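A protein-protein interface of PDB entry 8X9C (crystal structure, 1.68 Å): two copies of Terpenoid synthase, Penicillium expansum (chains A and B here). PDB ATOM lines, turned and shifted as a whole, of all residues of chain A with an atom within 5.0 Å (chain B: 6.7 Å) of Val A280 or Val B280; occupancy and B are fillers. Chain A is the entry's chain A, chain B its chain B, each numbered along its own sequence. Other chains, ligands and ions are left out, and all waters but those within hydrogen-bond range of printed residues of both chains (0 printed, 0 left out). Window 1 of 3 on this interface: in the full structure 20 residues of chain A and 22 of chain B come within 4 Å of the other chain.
SD of Met B273 sits at hydrogen-bond distance from N of Val A278, 3.7 Å away. O of Gly A277 lies close to SD of Met B273 (3.5 Å). OG of Ser A284 sits close to O of Pro B29, at 2.3 Å.
The backbone carbonyl oxygen of Val B280 lies within hydrogen-bond range of the side-chain hydroxyl of Ser B284, 3.1 Å away.
Among the printed residues, merely in contact across the chains: Gly A277 with Leu B276 (3.5 Å), Leu A276 with Gly B277 (3.6 Å), Val A280 with Phe B32 (3.7 Å), Phe A32 with Val B280 (3.8 Å), Glu A281 with Tyr B239 (3.8 Å), Val A280 with Val B280 (3.8 Å), Gly A277 with Gly B277 (3.8 Å), Val A280 with Leu B276 (3.9 Å) and Leu A276 with Val B280 (3.9 Å).
Of chain B, only Phe B32, Leu B276 and Val B280 come within 4 Å of Val A280. Of the printed residues of chain B, Phe A32 touches Val B280 (3.8 Å). Printed residues of chain A within 4 Å of Met B273: Gly A277 and Val A278. Of the printed residues of chain A, Leu B276 touches Gly A277 (3.5 Å) and Val A280 (3.9 Å). Printed residues of chain B within 4 Å of Gly A277: Met B273, Leu B276 and Gly B277. Of the printed residues of chain A, Phe B32 touches Val A280 (3.7 Å). Val B278 touches none of the printed residues of chain A. The nearest printed residue of chain B that does not touch Phe A32 is Arg B34 (4.2 Å).
Of the 17 printed residues of chain B, 7 touch a printed residue of chain A. Printed residues of chain B that touch a printed residue of chain A: Pro B29, Phe B32, Tyr B239, Met B273, Leu B276, Gly B277 and Val B280. Along chain B the printed residues that touch a printed residue of chain A span positions 29 to 280. Among the printed residues, no Asp or Glu carboxylate lies within 4 Å of a Lys or Arg side-chain nitrogen of the other chain.
Leu A276 touches Gly B277, and with the chains exchanged Gly A277 touches Leu B276. Leu A276 touches Val B280, and with the chains exchanged Val A280 touches Leu B276. Gly B277 touches its own counterpart, Gly A277. Val A280 touches its own counterpart, Val B280. Of the 12 pairs that touch across the chains among the printed residues, 8 have their exchanged pair printed and touching as well.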
ATOM      1  N   PHE A  32     -17.930 -32.175   4.483  1.00  0.00           N
ATOM      2  CA  PHE A  32     -18.672 -30.922   4.399  1.00  0.00           C
ATOM      3  C   PHE A  32     -20.169 -31.111   4.198  1.00  0.00           C
ATOM      4  O   PHE A  32     -20.899 -30.115   4.189  1.00  0.00           O
ATOM      5  CB  PHE A  32     -18.146 -30.041   3.247  1.00  0.00           C
ATOM      6  CG  PHE A  32     -18.282 -30.687   1.883  1.00  0.00           C
ATOM      7  CD1 PHE A  32     -19.445 -30.524   1.141  1.00  0.00           C
ATOM      8  CD2 PHE A  32     -17.262 -31.443   1.355  1.00  0.00           C
ATOM      9  CE1 PHE A  32     -19.585 -31.136  -0.108  1.00  0.00           C
ATOM     10  CE2 PHE A  32     -17.386 -32.042   0.101  1.00  0.00           C
ATOM     11  CZ  PHE A  32     -18.553 -31.880  -0.628  1.00  0.00           C
ATOM     12  N   LEU A 276     -17.239 -26.991  -5.660  1.00  0.00           N
ATOM     13  CA  LEU A 276     -17.714 -27.124  -4.285  1.00  0.00           C
ATOM     14  C   LEU A 276     -18.965 -26.285  -4.058  1.00  0.00           C
ATOM     15  O   LEU A 276     -19.921 -26.741  -3.419  1.00  0.00           O
ATOM     16  CB  LEU A 276     -16.610 -26.706  -3.314  1.00  0.00           C
ATOM     17  CG  LEU A 276     -16.843 -26.985  -1.821  1.00  0.00           C
ATOM     18  CD1 LEU A 276     -17.329 -28.413  -1.572  1.00  0.00           C
ATOM     19  CD2 LEU A 276     -15.596 -26.669  -1.010  1.00  0.00           C
ATOM     20  N   GLY A 277     -18.975 -25.053  -4.569  1.00  0.00           N
ATOM     21  CA  GLY A 277     -20.170 -24.231  -4.459  1.00  0.00           C
ATOM     22  C   GLY A 277     -21.368 -24.879  -5.122  1.00  0.00           C
ATOM     23  O   GLY A 277     -22.466 -24.914  -4.564  1.00  0.00           O
ATOM     24  N   VAL A 278     -21.168 -25.417  -6.325  1.00  0.00           N
ATOM     25  CA  VAL A 278     -22.252 -26.111  -7.014  1.00  0.00           C
ATOM     26  C   VAL A 278     -22.790 -27.256  -6.166  1.00  0.00           C
ATOM     27  O   VAL A 278     -24.004 -27.452  -6.070  1.00  0.00           O
ATOM     28  CB  VAL A 278     -21.780 -26.599  -8.396  1.00  0.00           C
ATOM     29  CG1 VAL A 278     -22.808 -27.565  -8.988  1.00  0.00           C
ATOM     30  CG2 VAL A 278     -21.554 -25.413  -9.326  1.00  0.00           C
ATOM     31  N   ILE A 279     -21.902 -28.042  -5.562  1.00  0.00           N
ATOM     32  CA  ILE A 279     -22.332 -29.187  -4.761  1.00  0.00           C
ATOM     33  C   ILE A 279     -23.167 -28.729  -3.572  1.00  0.00           C
ATOM     34  O   ILE A 279     -24.230 -29.301  -3.262  1.00  0.00           O
ATOM     35  CB  ILE A 279     -21.110 -29.988  -4.279  1.00  0.00           C
ATOM     36  CG1 ILE A 279     -20.374 -30.657  -5.442  1.00  0.00           C
ATOM     37  CG2 ILE A 279     -21.525 -31.023  -3.234  1.00  0.00           C
ATOM     38  CD1 ILE A 279     -18.941 -31.036  -5.058  1.00  0.00           C
ATOM     39  N   VAL A 280     -22.690 -27.700  -2.883  1.00  0.00           N
ATOM     40  CA  VAL A 280     -23.395 -27.254  -1.645  1.00  0.00           C
ATOM     41  C   VAL A 280     -24.781 -26.711  -2.019  1.00  0.00           C
ATOM     42  O   VAL A 280     -25.741 -26.991  -1.306  1.00  0.00           O
ATOM     43  CB  VAL A 280     -22.549 -26.226  -0.870  1.00  0.00           C
ATOM     44  CG1 VAL A 280     -23.317 -25.595   0.277  1.00  0.00           C
ATOM     45  CG2 VAL A 280     -21.253 -26.843  -0.373  1.00  0.00           C
ATOM     46  N   GLU A 281     -24.858 -25.983  -3.120  1.00  0.00           N
ATOM     47  CA  GLU A 281     -26.158 -25.460  -3.595  1.00  0.00           C
ATOM     48  C   GLU A 281     -27.088 -26.622  -3.965  1.00  0.00           C
ATOM     49  O   GLU A 281     -28.268 -26.549  -3.660  1.00  0.00           O
ATOM     50  CB  GLU A 281     -25.923 -24.541  -4.790  1.00  0.00           C
ATOM     51  CG  GLU A 281     -27.194 -23.919  -5.334  1.00  0.00           C
ATOM     52  CD  GLU A 281     -28.105 -23.356  -4.261  1.00  0.00           C
ATOM     53  OE1 GLU A 281     -27.795 -22.276  -3.735  1.00  0.00           O
ATOM     54  OE2 GLU A 281     -29.120 -24.002  -3.950  1.00  0.00           O
ATOM     55  N   GLN A 282     -26.551 -27.664  -4.586  1.00  0.00           N
ATOM     56  CA  GLN A 282     -27.393 -28.840  -4.921  1.00  0.00           C
ATOM     57  C   GLN A 282     -27.859 -29.515  -3.631  1.00  0.00           C
ATOM     58  O   GLN A 282     -28.997 -29.986  -3.603  1.00  0.00           O
ATOM     59  CB  GLN A 282     -26.677 -29.841  -5.826  1.00  0.00           C
ATOM     60  CG  GLN A 282     -26.519 -29.367  -7.260  1.00  0.00           C
ATOM     61  CD  GLN A 282     -27.850 -29.215  -7.950  1.00  0.00           C
ATOM     62  OE1 GLN A 282     -28.587 -30.177  -8.137  1.00  0.00           O
ATOM     63  NE2 GLN A 282     -28.166 -27.992  -8.336  1.00  0.00           N
ATOM     64  N   GLU A 283     -27.001 -29.542  -2.615  1.00  0.00           N
ATOM     65  CA  GLU A 283     -27.449 -30.115  -1.352  1.00  0.00           C
ATOM     66  C   GLU A 283     -28.575 -29.270  -0.760  1.00  0.00           C
ATOM     67  O   GLU A 283     -29.547 -29.805  -0.212  1.00  0.00           O
ATOM     68  CB  GLU A 283     -26.279 -30.226  -0.362  1.00  0.00           C
ATOM     69  CG  GLU A 283     -25.348 -31.431  -0.613  1.00  0.00           C
ATOM     70  CD  GLU A 283     -24.486 -31.812   0.586  1.00  0.00           C
ATOM     71  OE1 GLU A 283     -24.477 -31.069   1.598  1.00  0.00           O
ATOM     72  OE2 GLU A 283     -23.864 -32.903   0.555  1.00  0.00           O
ATOM     73  N   SER A 284     -28.461 -27.941  -0.880  1.00  0.00           N
ATOM     74  CA  SER A 284     -29.533 -27.045  -0.454  1.00  0.00           C
ATOM     75  C   SER A 284     -30.788 -27.223  -1.302  1.00  0.00           C
ATOM     76  O   SER A 284     -31.906 -27.257  -0.769  1.00  0.00           O
ATOM     77  CB  SER A 284     -29.044 -25.596  -0.524  1.00  0.00           C
ATOM     78  OG  SER A 284     -29.882 -24.764   0.243  1.00  0.00           O
ATOM     79  N   PRO B  29     -33.201 -24.969   4.600  1.00  0.00           N
ATOM     80  CA  PRO B  29     -32.451 -25.472   3.441  1.00  0.00           C
ATOM     81  C   PRO B  29     -31.307 -24.570   2.988  1.00  0.00           C
ATOM     82  O   PRO B  29     -30.290 -25.083   2.510  1.00  0.00           O
ATOM     83  CB  PRO B  29     -33.536 -25.609   2.365  1.00  0.00           C
ATOM     84  CG  PRO B  29     -34.779 -25.913   3.143  1.00  0.00           C
ATOM     85  CD  PRO B  29     -34.659 -25.009   4.374  1.00  0.00           C
ATOM     86  N   PHE B  32     -26.102 -23.560   5.282  1.00  0.00           N
ATOM     87  CA  PHE B  32     -25.111 -24.533   4.839  1.00  0.00           C
ATOM     88  C   PHE B  32     -23.964 -24.768   5.820  1.00  0.00           C
ATOM     89  O   PHE B  32     -23.128 -25.650   5.573  1.00  0.00           O
ATOM     90  CB  PHE B  32     -24.524 -24.096   3.491  1.00  0.00           C
ATOM     91  CG  PHE B  32     -23.769 -22.796   3.561  1.00  0.00           C
ATOM     92  CD1 PHE B  32     -22.443 -22.767   3.959  1.00  0.00           C
ATOM     93  CD2 PHE B  32     -24.380 -21.612   3.194  1.00  0.00           C
ATOM     94  CE1 PHE B  32     -21.749 -21.568   4.015  1.00  0.00           C
ATOM     95  CE2 PHE B  32     -23.693 -20.404   3.243  1.00  0.00           C
ATOM     96  CZ  PHE B  32     -22.374 -20.382   3.654  1.00  0.00           C
ATOM     97  N   ARG B  34     -21.401 -25.859   8.728  1.00  0.00           N
ATOM     98  CA  ARG B  34     -21.161 -27.014   9.583  1.00  0.00           C
ATOM     99  C   ARG B  34     -21.222 -26.669  11.064  1.00  0.00           C
ATOM    100  O   ARG B  34     -21.248 -27.581  11.904  1.00  0.00           O
ATOM    101  CB  ARG B  34     -19.790 -27.619   9.279  1.00  0.00           C
ATOM    102  CG  ARG B  34     -18.646 -26.759   9.778  1.00  0.00           C
ATOM    103  CD  ARG B  34     -17.278 -27.161   9.224  1.00  0.00           C
ATOM    104  NE  ARG B  34     -16.806 -28.436   9.743  1.00  0.00           N
ATOM    105  CZ  ARG B  34     -16.489 -29.481   8.988  1.00  0.00           C
ATOM    106  NH1 ARG B  34     -16.479 -29.400   7.665  1.00  0.00           N
ATOM    107  NH2 ARG B  34     -16.110 -30.613   9.574  1.00  0.00           N
ATOM    108  N   VAL B 232     -14.746 -17.026   7.219  1.00  0.00           N
ATOM    109  CA  VAL B 232     -16.096 -17.570   7.081  1.00  0.00           C
ATOM    110  C   VAL B 232     -17.140 -16.497   7.354  1.00  0.00           C
ATOM    111  O   VAL B 232     -18.109 -16.332   6.604  1.00  0.00           O
ATOM    112  CB  VAL B 232     -16.288 -18.768   8.024  1.00  0.00           C
ATOM    113  CG1 VAL B 232     -17.729 -19.250   7.944  1.00  0.00           C
ATOM    114  CG2 VAL B 232     -15.322 -19.898   7.647  1.00  0.00           C
ATOM    115  N   TYR B 239     -21.803 -13.493   0.747  1.00  0.00           N
ATOM    116  CA  TYR B 239     -22.561 -14.449  -0.052  1.00  0.00           C
ATOM    117  C   TYR B 239     -24.051 -14.141   0.012  1.00  0.00           C
ATOM    118  O   TYR B 239     -24.728 -14.077  -1.019  1.00  0.00           O
ATOM    119  CB  TYR B 239     -22.273 -15.877   0.415  1.00  0.00           C
ATOM    120  CG  TYR B 239     -23.059 -16.921  -0.347  1.00  0.00           C
ATOM    121  CD1 TYR B 239     -22.601 -17.383  -1.574  1.00  0.00           C
ATOM    122  CD2 TYR B 239     -24.239 -17.450   0.163  1.00  0.00           C
ATOM    123  CE1 TYR B 239     -23.304 -18.342  -2.283  1.00  0.00           C
ATOM    124  CE2 TYR B 239     -24.951 -18.405  -0.541  1.00  0.00           C
ATOM    125  CZ  TYR B 239     -24.472 -18.839  -1.759  1.00  0.00           C
ATOM    126  OH  TYR B 239     -25.179 -19.794  -2.460  1.00  0.00           O
ATOM    127  N   MET B 273     -20.757 -18.985  -6.993  1.00  0.00           N
ATOM    128  CA  MET B 273     -20.482 -20.369  -6.647  1.00  0.00           C
ATOM    129  C   MET B 273     -19.054 -20.529  -6.144  1.00  0.00           C
ATOM    130  O   MET B 273     -18.812 -21.295  -5.205  1.00  0.00           O
ATOM    131  CB  MET B 273     -20.757 -21.284  -7.846  1.00  0.00           C
ATOM    132  CG  MET B 273     -22.243 -21.421  -8.106  1.00  0.00           C
ATOM    133  SD  MET B 273     -23.095 -22.329  -6.805  1.00  0.00           S
ATOM    134  CE  MET B 273     -23.844 -20.973  -5.885  1.00  0.00           C
ATOM    135  N   LEU B 275     -17.375 -18.267  -4.481  1.00  0.00           N
ATOM    136  CA  LEU B 275     -17.355 -17.730  -3.125  1.00  0.00           C
ATOM    137  C   LEU B 275     -17.863 -18.762  -2.127  1.00  0.00           C
ATOM    138  O   LEU B 275     -17.289 -18.939  -1.049  1.00  0.00           O
ATOM    139  CB  LEU B 275     -18.219 -16.478  -3.045  1.00  0.00           C
ATOM    140  CG  LEU B 275     -18.188 -15.772  -1.687  1.00  0.00           C
ATOM    141  CD1 LEU B 275     -16.750 -15.441  -1.274  1.00  0.00           C
ATOM    142  CD2 LEU B 275     -19.064 -14.544  -1.710  1.00  0.00           C
ATOM    143  N   LEU B 276     -18.975 -19.424  -2.457  1.00  0.00           N
ATOM    144  CA  LEU B 276     -19.507 -20.446  -1.565  1.00  0.00           C
ATOM    145  C   LEU B 276     -18.477 -21.545  -1.330  1.00  0.00           C
ATOM    146  O   LEU B 276     -18.298 -22.004  -0.200  1.00  0.00           O
ATOM    147  CB  LEU B 276     -20.799 -21.018  -2.154  1.00  0.00           C
ATOM    148  CG  LEU B 276     -21.545 -22.058  -1.317  1.00  0.00           C
ATOM    149  CD1 LEU B 276     -21.887 -21.432   0.053  1.00  0.00           C
ATOM    150  CD2 LEU B 276     -22.800 -22.521  -2.012  1.00  0.00           C
ATOM    151  N   GLY B 277     -17.804 -22.008  -2.396  1.00  0.00           N
ATOM    152  CA  GLY B 277     -16.725 -22.968  -2.207  1.00  0.00           C
ATOM    153  C   GLY B 277     -15.630 -22.446  -1.285  1.00  0.00           C
ATOM    154  O   GLY B 277     -15.146 -23.165  -0.409  1.00  0.00           O
ATOM    155  N   VAL B 278     -15.218 -21.192  -1.473  1.00  0.00           N
ATOM    156  CA  VAL B 278     -14.178 -20.629  -0.609  1.00  0.00           C
ATOM    157  C   VAL B 278     -14.629 -20.644   0.847  1.00  0.00           C
ATOM    158  O   VAL B 278     -13.864 -21.021   1.743  1.00  0.00           O
ATOM    159  CB  VAL B 278     -13.805 -19.213  -1.084  1.00  0.00           C
ATOM    160  CG1 VAL B 278     -12.931 -18.501  -0.054  1.00  0.00           C
ATOM    161  CG2 VAL B 278     -13.095 -19.276  -2.433  1.00  0.00           C
ATOM    162  N   ILE B 279     -15.891 -20.279   1.099  1.00  0.00           N
ATOM    163  CA  ILE B 279     -16.429 -20.289   2.463  1.00  0.00           C
ATOM    164  C   ILE B 279     -16.386 -21.692   3.053  1.00  0.00           C
ATOM    165  O   ILE B 279     -15.921 -21.898   4.179  1.00  0.00           O
ATOM    166  CB  ILE B 279     -17.866 -19.731   2.488  1.00  0.00           C
ATOM    167  CG1 ILE B 279     -17.889 -18.266   2.058  1.00  0.00           C
ATOM    168  CG2 ILE B 279     -18.500 -19.900   3.880  1.00  0.00           C
ATOM    169  CD1 ILE B 279     -19.271 -17.806   1.612  1.00  0.00           C
ATOM    170  N   VAL B 280     -16.894 -22.679   2.309  1.00  0.00           N
ATOM    171  CA  VAL B 280     -16.945 -24.041   2.834  1.00  0.00           C
ATOM    172  C   VAL B 280     -15.540 -24.566   3.103  1.00  0.00           C
ATOM    173  O   VAL B 280     -15.294 -25.234   4.111  1.00  0.00           O
ATOM    174  CB  VAL B 280     -17.725 -24.946   1.862  1.00  0.00           C
ATOM    175  CG1 VAL B 280     -17.698 -26.397   2.322  1.00  0.00           C
ATOM    176  CG2 VAL B 280     -19.155 -24.439   1.766  1.00  0.00           C
ATOM    177  N   GLU B 281     -14.602 -24.282   2.197  1.00  0.00           N
ATOM    178  CA  GLU B 281     -13.207 -24.663   2.412  1.00  0.00           C
ATOM    179  C   GLU B 281     -12.647 -24.001   3.672  1.00  0.00           C
ATOM    180  O   GLU B 281     -11.886 -24.621   4.429  1.00  0.00           O
ATOM    181  CB  GLU B 281     -12.383 -24.247   1.202  1.00  0.00           C
ATOM    182  CG  GLU B 281     -10.901 -24.150   1.474  1.00  0.00           C
ATOM    183  CD  GLU B 281     -10.293 -22.997   0.699  1.00  0.00           C
ATOM    184  OE1 GLU B 281     -10.536 -21.815   1.120  1.00  0.00           O
ATOM    185  OE2 GLU B 281      -9.639 -23.242  -0.334  1.00  0.00           O
ATOM    186  N   GLN B 282     -13.022 -22.741   3.922  1.00  0.00           N
ATOM    187  CA  GLN B 282     -12.541 -22.060   5.128  1.00  0.00           C
ATOM    188  C   GLN B 282     -13.147 -22.669   6.392  1.00  0.00           C
ATOM    189  O   GLN B 282     -12.471 -22.779   7.424  1.00  0.00           O
ATOM    190  CB  GLN B 282     -12.847 -20.555   5.059  1.00  0.00           C
ATOM    191  CG  GLN B 282     -11.928 -19.744   4.147  1.00  0.00           C
ATOM    192  CD  GLN B 282     -10.458 -19.861   4.520  1.00  0.00           C
ATOM    193  OE1 GLN B 282     -10.036 -19.397   5.582  1.00  0.00           O
ATOM    194  NE2 GLN B 282      -9.663 -20.456   3.625  1.00  0.00           N
ATOM    195  N   GLU B 283     -14.418 -23.079   6.330  1.00  0.00           N
ATOM    196  CA  GLU B 283     -15.006 -23.794   7.461  1.00  0.00           C
ATOM    197  C   GLU B 283     -14.251 -25.091   7.724  1.00  0.00           C
ATOM    198  O   GLU B 283     -13.979 -25.430   8.876  1.00  0.00           O
ATOM    199  CB  GLU B 283     -16.492 -24.069   7.202  1.00  0.00           C
ATOM    200  CG  GLU B 283     -17.389 -22.834   7.294  1.00  0.00           C
ATOM    201  CD  GLU B 283     -18.847 -23.145   7.628  1.00  0.00           C
ATOM    202  OE1 GLU B 283     -19.277 -24.317   7.486  1.00  0.00           O
ATOM    203  OE2 GLU B 283     -19.569 -22.202   8.033  1.00  0.00           O
ATOM    204  N   SER B 284     -13.897 -25.843   6.664  1.00  0.00           N
ATOM    205  CA  SER B 284     -13.118 -27.064   6.877  1.00  0.00           C
ATOM    206  C   SER B 284     -11.722 -26.757   7.386  1.00  0.00           C
ATOM    207  O   SER B 284     -11.176 -27.513   8.196  1.00  0.00           O
ATOM    208  CB  SER B 284     -12.996 -27.894   5.580  1.00  0.00           C
ATOM    209  OG  SER B 284     -14.259 -28.073   4.971  1.00  0.00           O
ATOM    210  N   LEU B 285     -11.110 -25.685   6.881  1.00  0.00           N
ATOM    211  CA  LEU B 285      -9.773 -25.320   7.328  1.00  0.00           C
ATOM    212  C   LEU B 285      -9.774 -24.986   8.815  1.00  0.00           C
ATOM    213  O   LEU B 285      -8.906 -25.446   9.567  1.00  0.00           O
ATOM    214  CB  LEU B 285      -9.259 -24.136   6.508  1.00  0.00           C
ATOM    215  CG  LEU B 285      -7.950 -23.524   7.004  1.00  0.00           C
ATOM    216  CD1 LEU B 285      -6.841 -24.583   7.032  1.00  0.00           C
ATOM    217  CD2 LEU B 285      -7.550 -22.308   6.163  1.00  0.00           C
